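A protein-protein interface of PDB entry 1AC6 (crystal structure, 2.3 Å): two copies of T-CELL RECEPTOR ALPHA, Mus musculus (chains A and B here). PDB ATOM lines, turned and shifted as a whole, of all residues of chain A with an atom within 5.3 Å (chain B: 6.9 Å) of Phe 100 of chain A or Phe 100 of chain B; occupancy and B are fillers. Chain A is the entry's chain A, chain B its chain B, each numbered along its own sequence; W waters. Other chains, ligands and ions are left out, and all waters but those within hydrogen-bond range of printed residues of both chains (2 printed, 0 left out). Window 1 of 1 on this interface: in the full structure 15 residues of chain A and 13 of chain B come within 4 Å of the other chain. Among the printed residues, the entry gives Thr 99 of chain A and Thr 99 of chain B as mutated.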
ATOM      1  N   VAL A   3     -20.306 -19.760 -25.812  1.00  0.00           N
ATOM      2  CA  VAL A   3     -19.879 -19.115 -24.589  1.00  0.00           C
ATOM      3  C   VAL A   3     -20.261 -17.626 -24.651  1.00  0.00           C
ATOM      4  O   VAL A   3     -20.216 -17.025 -25.731  1.00  0.00           O
ATOM      5  CB  VAL A   3     -18.344 -19.299 -24.386  1.00  0.00           C
ATOM      6  CG1 VAL A   3     -17.832 -18.431 -23.276  1.00  0.00           C
ATOM      7  CG2 VAL A   3     -18.029 -20.765 -24.091  1.00  0.00           C
ATOM      8  N   TYR A  35      -8.755 -18.955 -19.766  1.00  0.00           N
ATOM      9  CA  TYR A  35      -7.432 -18.710 -20.349  1.00  0.00           C
ATOM     10  C   TYR A  35      -7.134 -17.236 -20.193  1.00  0.00           C
ATOM     11  O   TYR A  35      -8.053 -16.415 -20.172  1.00  0.00           O
ATOM     12  CB  TYR A  35      -7.380 -19.059 -21.844  1.00  0.00           C
ATOM     13  CG  TYR A  35      -7.134 -20.520 -22.214  1.00  0.00           C
ATOM     14  CD1 TYR A  35      -8.012 -21.528 -21.798  1.00  0.00           C
ATOM     15  CD2 TYR A  35      -6.060 -20.883 -23.051  1.00  0.00           C
ATOM     16  CE1 TYR A  35      -7.842 -22.860 -22.205  1.00  0.00           C
ATOM     17  CE2 TYR A  35      -5.881 -22.211 -23.476  1.00  0.00           C
ATOM     18  CZ  TYR A  35      -6.779 -23.200 -23.045  1.00  0.00           C
ATOM     19  OH  TYR A  35      -6.648 -24.516 -23.462  1.00  0.00           O
ATOM     20  N   GLY A  42      -0.312 -14.910 -26.737  1.00  0.00           N
ATOM     21  CA  GLY A  42      -1.482 -15.675 -27.127  1.00  0.00           C
ATOM     22  C   GLY A  42      -2.187 -16.153 -25.862  1.00  0.00           C
ATOM     23  O   GLY A  42      -1.633 -15.991 -24.765  1.00  0.00           O
ATOM     24  N   PRO A  43      -3.413 -16.706 -25.956  1.00  0.00           N
ATOM     25  CA  PRO A  43      -4.120 -17.176 -24.763  1.00  0.00           C
ATOM     26  C   PRO A  43      -3.312 -18.255 -24.057  1.00  0.00           C
ATOM     27  O   PRO A  43      -2.702 -19.098 -24.716  1.00  0.00           O
ATOM     28  CB  PRO A  43      -5.393 -17.771 -25.355  1.00  0.00           C
ATOM     29  CG  PRO A  43      -5.600 -16.969 -26.610  1.00  0.00           C
ATOM     30  CD  PRO A  43      -4.207 -16.970 -27.164  1.00  0.00           C
ATOM     31  N   TYR A  88     -10.702 -15.050 -21.240  1.00  0.00           N
ATOM     32  CA  TYR A  88     -11.673 -15.726 -22.122  1.00  0.00           C
ATOM     33  C   TYR A  88     -12.197 -16.924 -21.380  1.00  0.00           C
ATOM     34  O   TYR A  88     -11.434 -17.633 -20.728  1.00  0.00           O
ATOM     35  CB  TYR A  88     -11.038 -16.318 -23.394  1.00  0.00           C
ATOM     36  CG  TYR A  88     -10.425 -15.344 -24.373  1.00  0.00           C
ATOM     37  CD1 TYR A  88     -11.201 -14.712 -25.328  1.00  0.00           C
ATOM     38  CD2 TYR A  88      -9.067 -15.050 -24.322  1.00  0.00           C
ATOM     39  CE1 TYR A  88     -10.640 -13.809 -26.209  1.00  0.00           C
ATOM     40  CE2 TYR A  88      -8.509 -14.158 -25.187  1.00  0.00           C
ATOM     41  CZ  TYR A  88      -9.296 -13.540 -26.125  1.00  0.00           C
ATOM     42  OH  TYR A  88      -8.715 -12.633 -26.960  1.00  0.00           O
ATOM     43  N   CYS A  89     -13.487 -17.175 -21.514  1.00  0.00           N
ATOM     44  CA  CYS A  89     -14.092 -18.330 -20.887  1.00  0.00           C
ATOM     45  C   CYS A  89     -14.196 -19.288 -22.037  1.00  0.00           C
ATOM     46  O   CYS A  89     -14.471 -18.860 -23.149  1.00  0.00           O
ATOM     47  CB  CYS A  89     -15.461 -17.973 -20.351  1.00  0.00           C
ATOM     48  SG  CYS A  89     -16.379 -19.334 -19.583  1.00  0.00           S
ATOM     49  N   ALA A  90     -13.963 -20.570 -21.787  1.00  0.00           N
ATOM     50  CA  ALA A  90     -13.987 -21.548 -22.845  1.00  0.00           C
ATOM     51  C   ALA A  90     -14.589 -22.885 -22.413  1.00  0.00           C
ATOM     52  O   ALA A  90     -14.785 -23.133 -21.226  1.00  0.00           O
ATOM     53  CB  ALA A  90     -12.601 -21.726 -23.348  1.00  0.00           C
ATOM     54  N   LEU A  98     -11.882 -26.261 -29.054  1.00  0.00           N
ATOM     55  CA  LEU A  98     -12.140 -25.300 -27.987  1.00  0.00           C
ATOM     56  C   LEU A  98     -13.020 -24.134 -28.422  1.00  0.00           C
ATOM     57  O   LEU A  98     -12.767 -23.495 -29.444  1.00  0.00           O
ATOM     58  CB  LEU A  98     -10.815 -24.786 -27.424  1.00  0.00           C
ATOM     59  CG  LEU A  98     -10.611 -24.572 -25.926  1.00  0.00           C
ATOM     60  CD1 LEU A  98     -11.073 -25.777 -25.135  1.00  0.00           C
ATOM     61  CD2 LEU A  98      -9.127 -24.326 -25.659  1.00  0.00           C
ATOM     62  N   THR A  99     -14.077 -23.883 -27.660  1.00  0.00           N
ATOM     63  CA  THR A  99     -14.988 -22.781 -27.963  1.00  0.00           C
ATOM     64  C   THR A  99     -14.663 -21.630 -27.018  1.00  0.00           C
ATOM     65  O   THR A  99     -14.610 -21.824 -25.804  1.00  0.00           O
ATOM     66  CB  THR A  99     -16.462 -23.240 -27.843  1.00  0.00           C
ATOM     67  OG1 THR A  99     -16.730 -24.224 -28.855  1.00  0.00           O
ATOM     68  CG2 THR A  99     -17.421 -22.078 -28.020  1.00  0.00           C
ATOM     69  N   PHE A 100     -14.331 -20.470 -27.577  1.00  0.00           N
ATOM     70  CA  PHE A 100     -13.976 -19.310 -26.772  1.00  0.00           C
ATOM     71  C   PHE A 100     -15.068 -18.257 -26.777  1.00  0.00           C
ATOM     72  O   PHE A 100     -15.914 -18.218 -27.663  1.00  0.00           O
ATOM     73  CB  PHE A 100     -12.676 -18.649 -27.264  1.00  0.00           C
ATOM     74  CG  PHE A 100     -11.423 -19.430 -26.969  1.00  0.00           C
ATOM     75  CD1 PHE A 100     -11.032 -20.489 -27.795  1.00  0.00           C
ATOM     76  CD2 PHE A 100     -10.613 -19.087 -25.894  1.00  0.00           C
ATOM     77  CE1 PHE A 100      -9.846 -21.192 -27.548  1.00  0.00           C
ATOM     78  CE2 PHE A 100      -9.429 -19.776 -25.634  1.00  0.00           C
ATOM     79  CZ  PHE A 100      -9.041 -20.834 -26.461  1.00  0.00           C
ATOM     80  N   GLY A 101     -15.063 -17.443 -25.729  1.00  0.00           N
ATOM     81  CA  GLY A 101     -16.002 -16.357 -25.603  1.00  0.00           C
ATOM     82  C   GLY A 101     -15.291 -15.161 -26.195  1.00  0.00           C
ATOM     83  O   GLY A 101     -14.200 -15.297 -26.736  1.00  0.00           O
ATOM     84  N   ALA A 102     -15.870 -13.980 -26.067  1.00  0.00           N
ATOM     85  CA  ALA A 102     -15.260 -12.805 -26.674  1.00  0.00           C
ATOM     86  C   ALA A 102     -14.111 -12.209 -25.916  1.00  0.00           C
ATOM     87  O   ALA A 102     -13.292 -11.511 -26.500  1.00  0.00           O
ATOM     88  CB  ALA A 102     -16.307 -11.730 -26.957  1.00  0.00           C
ATOM     89  N   SER B   2       6.185 -25.642 -26.956  1.00  0.00           N
ATOM     90  CA  SER B   2       6.155 -24.248 -27.395  1.00  0.00           C
ATOM     91  C   SER B   2       5.763 -24.112 -28.868  1.00  0.00           C
ATOM     92  O   SER B   2       6.074 -24.975 -29.688  1.00  0.00           O
ATOM     93  CB  SER B   2       7.566 -23.650 -27.247  1.00  0.00           C
ATOM     94  OG  SER B   2       7.576 -22.472 -26.456  1.00  0.00           O
ATOM     95  N   VAL B   3       5.101 -23.011 -29.189  1.00  0.00           N
ATOM     96  CA  VAL B   3       4.715 -22.706 -30.554  1.00  0.00           C
ATOM     97  C   VAL B   3       5.278 -21.304 -30.848  1.00  0.00           C
ATOM     98  O   VAL B   3       5.220 -20.431 -29.976  1.00  0.00           O
ATOM     99  CB  VAL B   3       3.187 -22.728 -30.726  1.00  0.00           C
ATOM    100  CG1 VAL B   3       2.776 -21.798 -31.838  1.00  0.00           C
ATOM    101  CG2 VAL B   3       2.719 -24.131 -31.049  1.00  0.00           C
ATOM    102  N   THR B   4       5.861 -21.107 -32.034  1.00  0.00           N
ATOM    103  CA  THR B   4       6.418 -19.809 -32.427  1.00  0.00           C
ATOM    104  C   THR B   4       5.957 -19.469 -33.838  1.00  0.00           C
ATOM    105  O   THR B   4       6.146 -20.267 -34.755  1.00  0.00           O
ATOM    106  CB  THR B   4       7.948 -19.835 -32.404  1.00  0.00           C
ATOM    107  OG1 THR B   4       8.390 -20.689 -31.342  1.00  0.00           O
ATOM    108  CG2 THR B   4       8.508 -18.435 -32.157  1.00  0.00           C
ATOM    109  N   GLN B   5       5.344 -18.307 -34.033  1.00  0.00           N
ATOM    110  CA  GLN B   5       4.882 -17.963 -35.368  1.00  0.00           C
ATOM    111  C   GLN B   5       5.403 -16.617 -35.838  1.00  0.00           C
ATOM    112  O   GLN B   5       6.101 -15.941 -35.074  1.00  0.00           O
ATOM    113  CB  GLN B   5       3.342 -18.042 -35.476  1.00  0.00           C
ATOM    114  CG  GLN B   5       2.560 -17.146 -34.535  1.00  0.00           C
ATOM    115  CD  GLN B   5       1.057 -17.345 -34.643  1.00  0.00           C
ATOM    116  OE1 GLN B   5       0.459 -18.017 -33.814  1.00  0.00           O
ATOM    117  NE2 GLN B   5       0.443 -16.761 -35.666  1.00  0.00           N
ATOM    118  N   PHE B  33      -2.998 -26.971 -34.625  1.00  0.00           N
ATOM    119  CA  PHE B  33      -4.205 -26.206 -34.984  1.00  0.00           C
ATOM    120  C   PHE B  33      -3.872 -24.787 -35.389  1.00  0.00           C
ATOM    121  O   PHE B  33      -2.808 -24.246 -35.088  1.00  0.00           O
ATOM    122  CB  PHE B  33      -5.165 -26.012 -33.779  1.00  0.00           C
ATOM    123  CG  PHE B  33      -5.482 -27.256 -33.010  1.00  0.00           C
ATOM    124  CD1 PHE B  33      -4.557 -27.805 -32.127  1.00  0.00           C
ATOM    125  CD2 PHE B  33      -6.722 -27.867 -33.147  1.00  0.00           C
ATOM    126  CE1 PHE B  33      -4.863 -28.943 -31.389  1.00  0.00           C
ATOM    127  CE2 PHE B  33      -7.049 -29.018 -32.408  1.00  0.00           C
ATOM    128  CZ  PHE B  33      -6.119 -29.557 -31.532  1.00  0.00           C
ATOM    129  N   TRP B  34      -4.875 -24.172 -35.983  1.00  0.00           N
ATOM    130  CA  TRP B  34      -4.865 -22.761 -36.325  1.00  0.00           C
ATOM    131  C   TRP B  34      -6.273 -22.310 -35.921  1.00  0.00           C
ATOM    132  O   TRP B  34      -7.247 -23.047 -36.091  1.00  0.00           O
ATOM    133  CB  TRP B  34      -4.629 -22.486 -37.818  1.00  0.00           C
ATOM    134  CG  TRP B  34      -3.183 -22.394 -38.190  1.00  0.00           C
ATOM    135  CD1 TRP B  34      -2.414 -23.388 -38.711  1.00  0.00           C
ATOM    136  CD2 TRP B  34      -2.327 -21.249 -38.079  1.00  0.00           C
ATOM    137  NE1 TRP B  34      -1.134 -22.942 -38.930  1.00  0.00           N
ATOM    138  CE2 TRP B  34      -1.051 -21.630 -38.550  1.00  0.00           C
ATOM    139  CE3 TRP B  34      -2.515 -19.938 -37.625  1.00  0.00           C
ATOM    140  CZ2 TRP B  34       0.032 -20.752 -38.579  1.00  0.00           C
ATOM    141  CZ3 TRP B  34      -1.438 -19.066 -37.656  1.00  0.00           C
ATOM    142  CH2 TRP B  34      -0.180 -19.475 -38.130  1.00  0.00           C
ATOM    143  N   TYR B  35      -6.341 -21.148 -35.294  1.00  0.00           N
ATOM    144  CA  TYR B  35      -7.590 -20.528 -34.858  1.00  0.00           C
ATOM    145  C   TYR B  35      -7.544 -19.139 -35.478  1.00  0.00           C
ATOM    146  O   TYR B  35      -6.459 -18.624 -35.795  1.00  0.00           O
ATOM    147  CB  TYR B  35      -7.647 -20.374 -33.335  1.00  0.00           C
ATOM    148  CG  TYR B  35      -8.133 -21.581 -32.566  1.00  0.00           C
ATOM    149  CD1 TYR B  35      -7.431 -22.776 -32.596  1.00  0.00           C
ATOM    150  CD2 TYR B  35      -9.299 -21.518 -31.796  1.00  0.00           C
ATOM    151  CE1 TYR B  35      -7.870 -23.890 -31.885  1.00  0.00           C
ATOM    152  CE2 TYR B  35      -9.751 -22.629 -31.081  1.00  0.00           C
ATOM    153  CZ  TYR B  35      -9.028 -23.817 -31.135  1.00  0.00           C
ATOM    154  OH  TYR B  35      -9.457 -24.953 -30.479  1.00  0.00           O
ATOM    155  N   GLY B  42     -14.035 -13.607 -30.328  1.00  0.00           N
ATOM    156  CA  GLY B  42     -13.077 -14.461 -29.663  1.00  0.00           C
ATOM    157  C   GLY B  42     -12.374 -15.346 -30.672  1.00  0.00           C
ATOM    158  O   GLY B  42     -12.771 -15.379 -31.851  1.00  0.00           O
ATOM    159  N   PRO B  43     -11.308 -16.059 -30.261  1.00  0.00           N
ATOM    160  CA  PRO B  43     -10.608 -16.919 -31.210  1.00  0.00           C
ATOM    161  C   PRO B  43     -11.526 -18.055 -31.635  1.00  0.00           C
ATOM    162  O   PRO B  43     -12.353 -18.508 -30.848  1.00  0.00           O
ATOM    163  CB  PRO B  43      -9.439 -17.459 -30.380  1.00  0.00           C
ATOM    164  CG  PRO B  43      -9.267 -16.463 -29.265  1.00  0.00           C
ATOM    165  CD  PRO B  43     -10.687 -16.143 -28.925  1.00  0.00           C
ATOM    166  N   GLN B  44     -11.416 -18.493 -32.884  1.00  0.00           N
ATOM    167  CA  GLN B  44     -12.224 -19.608 -33.325  1.00  0.00           C
ATOM    168  C   GLN B  44     -11.464 -20.683 -34.093  1.00  0.00           C
ATOM    169  O   GLN B  44     -10.453 -20.431 -34.755  1.00  0.00           O
ATOM    170  CB  GLN B  44     -13.470 -19.154 -34.072  1.00  0.00           C
ATOM    171  CG  GLN B  44     -13.290 -18.640 -35.471  1.00  0.00           C
ATOM    172  CD  GLN B  44     -14.621 -18.178 -36.052  1.00  0.00           C
ATOM    173  OE1 GLN B  44     -15.327 -18.943 -36.725  1.00  0.00           O
ATOM    174  NE2 GLN B  44     -14.978 -16.930 -35.781  1.00  0.00           N
ATOM    175  N   PHE B  45     -11.918 -21.909 -33.903  1.00  0.00           N
ATOM    176  CA  PHE B  45     -11.326 -23.064 -34.545  1.00  0.00           C
ATOM    177  C   PHE B  45     -11.340 -22.888 -36.052  1.00  0.00           C
ATOM    178  O   PHE B  45     -12.349 -22.458 -36.624  1.00  0.00           O
ATOM    179  CB  PHE B  45     -12.107 -24.330 -34.123  1.00  0.00           C
ATOM    180  CG  PHE B  45     -11.603 -25.603 -34.745  1.00  0.00           C
ATOM    181  CD1 PHE B  45     -10.544 -26.304 -34.165  1.00  0.00           C
ATOM    182  CD2 PHE B  45     -12.173 -26.090 -35.913  1.00  0.00           C
ATOM    183  CE1 PHE B  45     -10.055 -27.464 -34.738  1.00  0.00           C
ATOM    184  CE2 PHE B  45     -11.697 -27.254 -36.504  1.00  0.00           C
ATOM    185  CZ  PHE B  45     -10.628 -27.945 -35.910  1.00  0.00           C
ATOM    186  N   TYR B  88      -3.788 -17.662 -34.855  1.00  0.00           N
ATOM    187  CA  TYR B  88      -2.923 -18.280 -33.859  1.00  0.00           C
ATOM    188  C   TYR B  88      -2.622 -19.701 -34.259  1.00  0.00           C
ATOM    189  O   TYR B  88      -3.458 -20.364 -34.871  1.00  0.00           O
ATOM    190  CB  TYR B  88      -3.581 -18.367 -32.478  1.00  0.00           C
ATOM    191  CG  TYR B  88      -3.982 -17.063 -31.877  1.00  0.00           C
ATOM    192  CD1 TYR B  88      -3.052 -16.271 -31.228  1.00  0.00           C
ATOM    193  CD2 TYR B  88      -5.291 -16.611 -31.968  1.00  0.00           C
ATOM    194  CE1 TYR B  88      -3.419 -15.038 -30.686  1.00  0.00           C
ATOM    195  CE2 TYR B  88      -5.661 -15.387 -31.430  1.00  0.00           C
ATOM    196  CZ  TYR B  88      -4.719 -14.613 -30.791  1.00  0.00           C
ATOM    197  OH  TYR B  88      -5.084 -13.413 -30.251  1.00  0.00           O
ATOM    198  N   CYS B  89      -1.468 -20.190 -33.821  1.00  0.00           N
ATOM    199  CA  CYS B  89      -1.070 -21.556 -34.074  1.00  0.00           C
ATOM    200  C   CYS B  89      -1.105 -22.161 -32.686  1.00  0.00           C
ATOM    201  O   CYS B  89      -0.647 -21.546 -31.726  1.00  0.00           O
ATOM    202  CB  CYS B  89       0.327 -21.612 -34.651  1.00  0.00           C
ATOM    203  SG  CYS B  89       0.794 -23.229 -35.300  1.00  0.00           S
ATOM    204  N   ALA B  90      -1.755 -23.311 -32.580  1.00  0.00           N
ATOM    205  CA  ALA B  90      -1.914 -23.983 -31.321  1.00  0.00           C
ATOM    206  C   ALA B  90      -1.336 -25.362 -31.407  1.00  0.00           C
ATOM    207  O   ALA B  90      -1.103 -25.894 -32.505  1.00  0.00           O
ATOM    208  CB  ALA B  90      -3.393 -24.055 -30.951  1.00  0.00           C
ATOM    209  N   LEU B  91      -1.199 -25.972 -30.238  1.00  0.00           N
ATOM    210  CA  LEU B  91      -0.638 -27.304 -30.117  1.00  0.00           C
ATOM    211  C   LEU B  91      -1.315 -27.953 -28.917  1.00  0.00           C
ATOM    212  O   LEU B  91      -1.564 -27.291 -27.912  1.00  0.00           O
ATOM    213  CB  LEU B  91       0.877 -27.166 -29.891  1.00  0.00           C
ATOM    214  CG  LEU B  91       1.838 -28.327 -29.692  1.00  0.00           C
ATOM    215  CD1 LEU B  91       3.261 -27.784 -29.783  1.00  0.00           C
ATOM    216  CD2 LEU B  91       1.601 -28.974 -28.335  1.00  0.00           C
ATOM    217  N   LEU B  98      -4.237 -26.620 -24.692  1.00  0.00           N
ATOM    218  CA  LEU B  98      -3.771 -26.027 -25.948  1.00  0.00           C
ATOM    219  C   LEU B  98      -2.763 -24.949 -25.639  1.00  0.00           C
ATOM    220  O   LEU B  98      -2.941 -24.170 -24.712  1.00  0.00           O
ATOM    221  CB  LEU B  98      -4.929 -25.415 -26.747  1.00  0.00           C
ATOM    222  CG  LEU B  98      -5.440 -26.195 -27.977  1.00  0.00           C
ATOM    223  CD1 LEU B  98      -6.017 -27.522 -27.550  1.00  0.00           C
ATOM    224  CD2 LEU B  98      -6.483 -25.396 -28.737  1.00  0.00           C
ATOM    225  N   THR B  99      -1.662 -24.958 -26.369  1.00  0.00           N
ATOM    226  CA  THR B  99      -0.600 -23.980 -26.189  1.00  0.00           C
ATOM    227  C   THR B  99      -0.641 -23.118 -27.418  1.00  0.00           C
ATOM    228  O   THR B  99      -0.611 -23.657 -28.523  1.00  0.00           O
ATOM    229  CB  THR B  99       0.743 -24.665 -26.119  1.00  0.00           C
ATOM    230  OG1 THR B  99       0.723 -25.579 -25.018  1.00  0.00           O
ATOM    231  CG2 THR B  99       1.868 -23.649 -25.930  1.00  0.00           C
ATOM    232  N   PHE B 100      -0.722 -21.800 -27.221  1.00  0.00           N
ATOM    233  CA  PHE B 100      -0.815 -20.814 -28.304  1.00  0.00           C
ATOM    234  C   PHE B 100       0.410 -19.991 -28.677  1.00  0.00           C
ATOM    235  O   PHE B 100       1.191 -19.573 -27.818  1.00  0.00           O
ATOM    236  CB  PHE B 100      -1.920 -19.801 -27.994  1.00  0.00           C
ATOM    237  CG  PHE B 100      -3.295 -20.297 -28.286  1.00  0.00           C
ATOM    238  CD1 PHE B 100      -4.023 -20.992 -27.314  1.00  0.00           C
ATOM    239  CD2 PHE B 100      -3.881 -20.065 -29.536  1.00  0.00           C
ATOM    240  CE1 PHE B 100      -5.305 -21.443 -27.582  1.00  0.00           C
ATOM    241  CE2 PHE B 100      -5.163 -20.510 -29.814  1.00  0.00           C
ATOM    242  CZ  PHE B 100      -5.879 -21.204 -28.836  1.00  0.00           C
ATOM    243  N   GLY B 101       0.533 -19.711 -29.970  1.00  0.00           N
ATOM    244  CA  GLY B 101       1.595 -18.839 -30.422  1.00  0.00           C
ATOM    245  C   GLY B 101       1.073 -17.447 -30.078  1.00  0.00           C
ATOM    246  O   GLY B 101      -0.074 -17.314 -29.650  1.00  0.00           O
ATOM    247  N   ALA B 102       1.839 -16.398 -30.355  1.00  0.00           N
ATOM    248  CA  ALA B 102       1.400 -15.046 -30.019  1.00  0.00           C
ATOM    249  C   ALA B 102       0.372 -14.440 -30.967  1.00  0.00           C
ATOM    250  O   ALA B 102      -0.333 -13.496 -30.597  1.00  0.00           O
ATOM    251  CB  ALA B 102       2.610 -14.125 -29.857  1.00  0.00           C
ATOM    252  N   GLY B 103       0.288 -14.994 -32.178  1.00  0.00           N
ATOM    253  CA  GLY B 103      -0.663 -14.523 -33.173  1.00  0.00           C
ATOM    254  C   GLY B 103      -0.066 -13.578 -34.186  1.00  0.00           C
ATOM    255  O   GLY B 103       0.893 -12.869 -33.891  1.00  0.00           O
HETATM  256  O   HOH W   1     -14.771 -20.131 -30.292  1.00  0.00           O
HETATM  257  O   HOH W   2      -0.434 -20.746 -24.647  1.00  0.00           O
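N of Leu 98 of chain B lies within hydrogen-bond range of OH of Tyr 35 of chain A, at 3.4 Å. N of Leu 98 of chain A lies within hydrogen-bond range of OH of Tyr 35 of chain B, at 3.1 Å.
The backbone NH (N) of Tyr 35 of chain A lies within hydrogen-bond range of the backbone carbonyl oxygen (O) of Tyr 88 of chain A (3.1 Å). The backbone carbonyl oxygen of Cys 89 of chain A sits at hydrogen-bond distance from the backbone NH of Gly 101 of chain A (3.0 Å). The backbone carbonyl oxygen (O) of Tyr 35 of chain B lies within hydrogen-bond range of the backbone NH (N) of Tyr 88 of chain B (3.0 Å). O of Cys 89 of chain B sits at hydrogen-bond distance from N of Gly 101 of chain B (2.8 Å).
Among the printed residues, merely in contact across the chains: Gly 42 of chain A with Gly 101 of chain B, Gly 42 of chain A with Ala 102 of chain B, Pro 43 of chain A with Phe 100 of chain B, Tyr 88 of chain A with Pro 43 of chain B, Phe 100 of chain A with Tyr 35 of chain B, Phe 100 of chain A with Pro 43 of chain B, Phe 100 of chain A with Phe 100 of chain B, Gly 101 of chain A with Gly 42 of chain B and Ala 102 of chain A with Gly 42 of chain B.
Of chain B, only Tyr 35, Pro 43 and Phe 100 come within 4 Å of Phe 100 of chain A. Of chain A, only Pro 43 and Phe 100 come within 4 Å of Phe 100 of chain B. Printed residues of chain B within 4 Å of Gly 101 of chain A: Gly 42 (3.2 Å). Of the printed residues of chain B, Leu 98 of chain A touches Tyr 35. Of the printed residues of chain A, Gly 42 of chain B touches Gly 101 and Ala 102. Printed residues of chain B within 4 Å of Ala 102 of chain A: Gly 42 (3.9 Å). Printed residues of chain B within 4 Å of Pro 43 of chain A: Phe 100. The nearest residue of chain B that does not touch Phe 100 of chain A is Gly 42 of chain B (4.8 Å).
Of the 21 printed residues of chain B, 7 touch a printed residue of chain A. Hydrophobic or aromatic side chains of chain B within 4 Å of the printed part of chain A: Tyr 35, Pro 43, Leu 98 and Phe 100.
Gly 42 of chain A touches Gly 101 of chain B, and with the chains exchanged Gly 101 of chain A touches Gly 42 of chain B. Gly 42 of chain A touches Ala 102 of chain B, and with the chains exchanged Ala 102 of chain A touches Gly 42 of chain B. Pro 43 of chain A touches Phe 100 of chain B, and with the chains exchanged Phe 100 of chain A touches Pro 43 of chain B. Tyr 88 of chain A touches Pro 43 of chain B, but with the chains exchanged Pro 43 of chain A does not touch Tyr 88 of chain B (4.1 Å). Positions printed for both chains: 3, 35, 42, 43, 88, 89, 90, 98, 99, 100, 101 and 102. Of the 11 pairs that touch across the chains among the printed residues, 9 have their exchanged pair printed and touching as well.
Water W1 lies within hydrogen-bond range of the backbone NH (N) of Phe 100 of chain A (2.8 Å) and the backbone carbonyl oxygen (O) of Pro 43 of chain B (3.0 Å). Water W2 lies within hydrogen-bond range of the backbone NH (N) of Phe 100 of chain B (2.8 Å) and the backbone carbonyl oxygen (O) of Pro 43 of chain A (2.8 Å).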
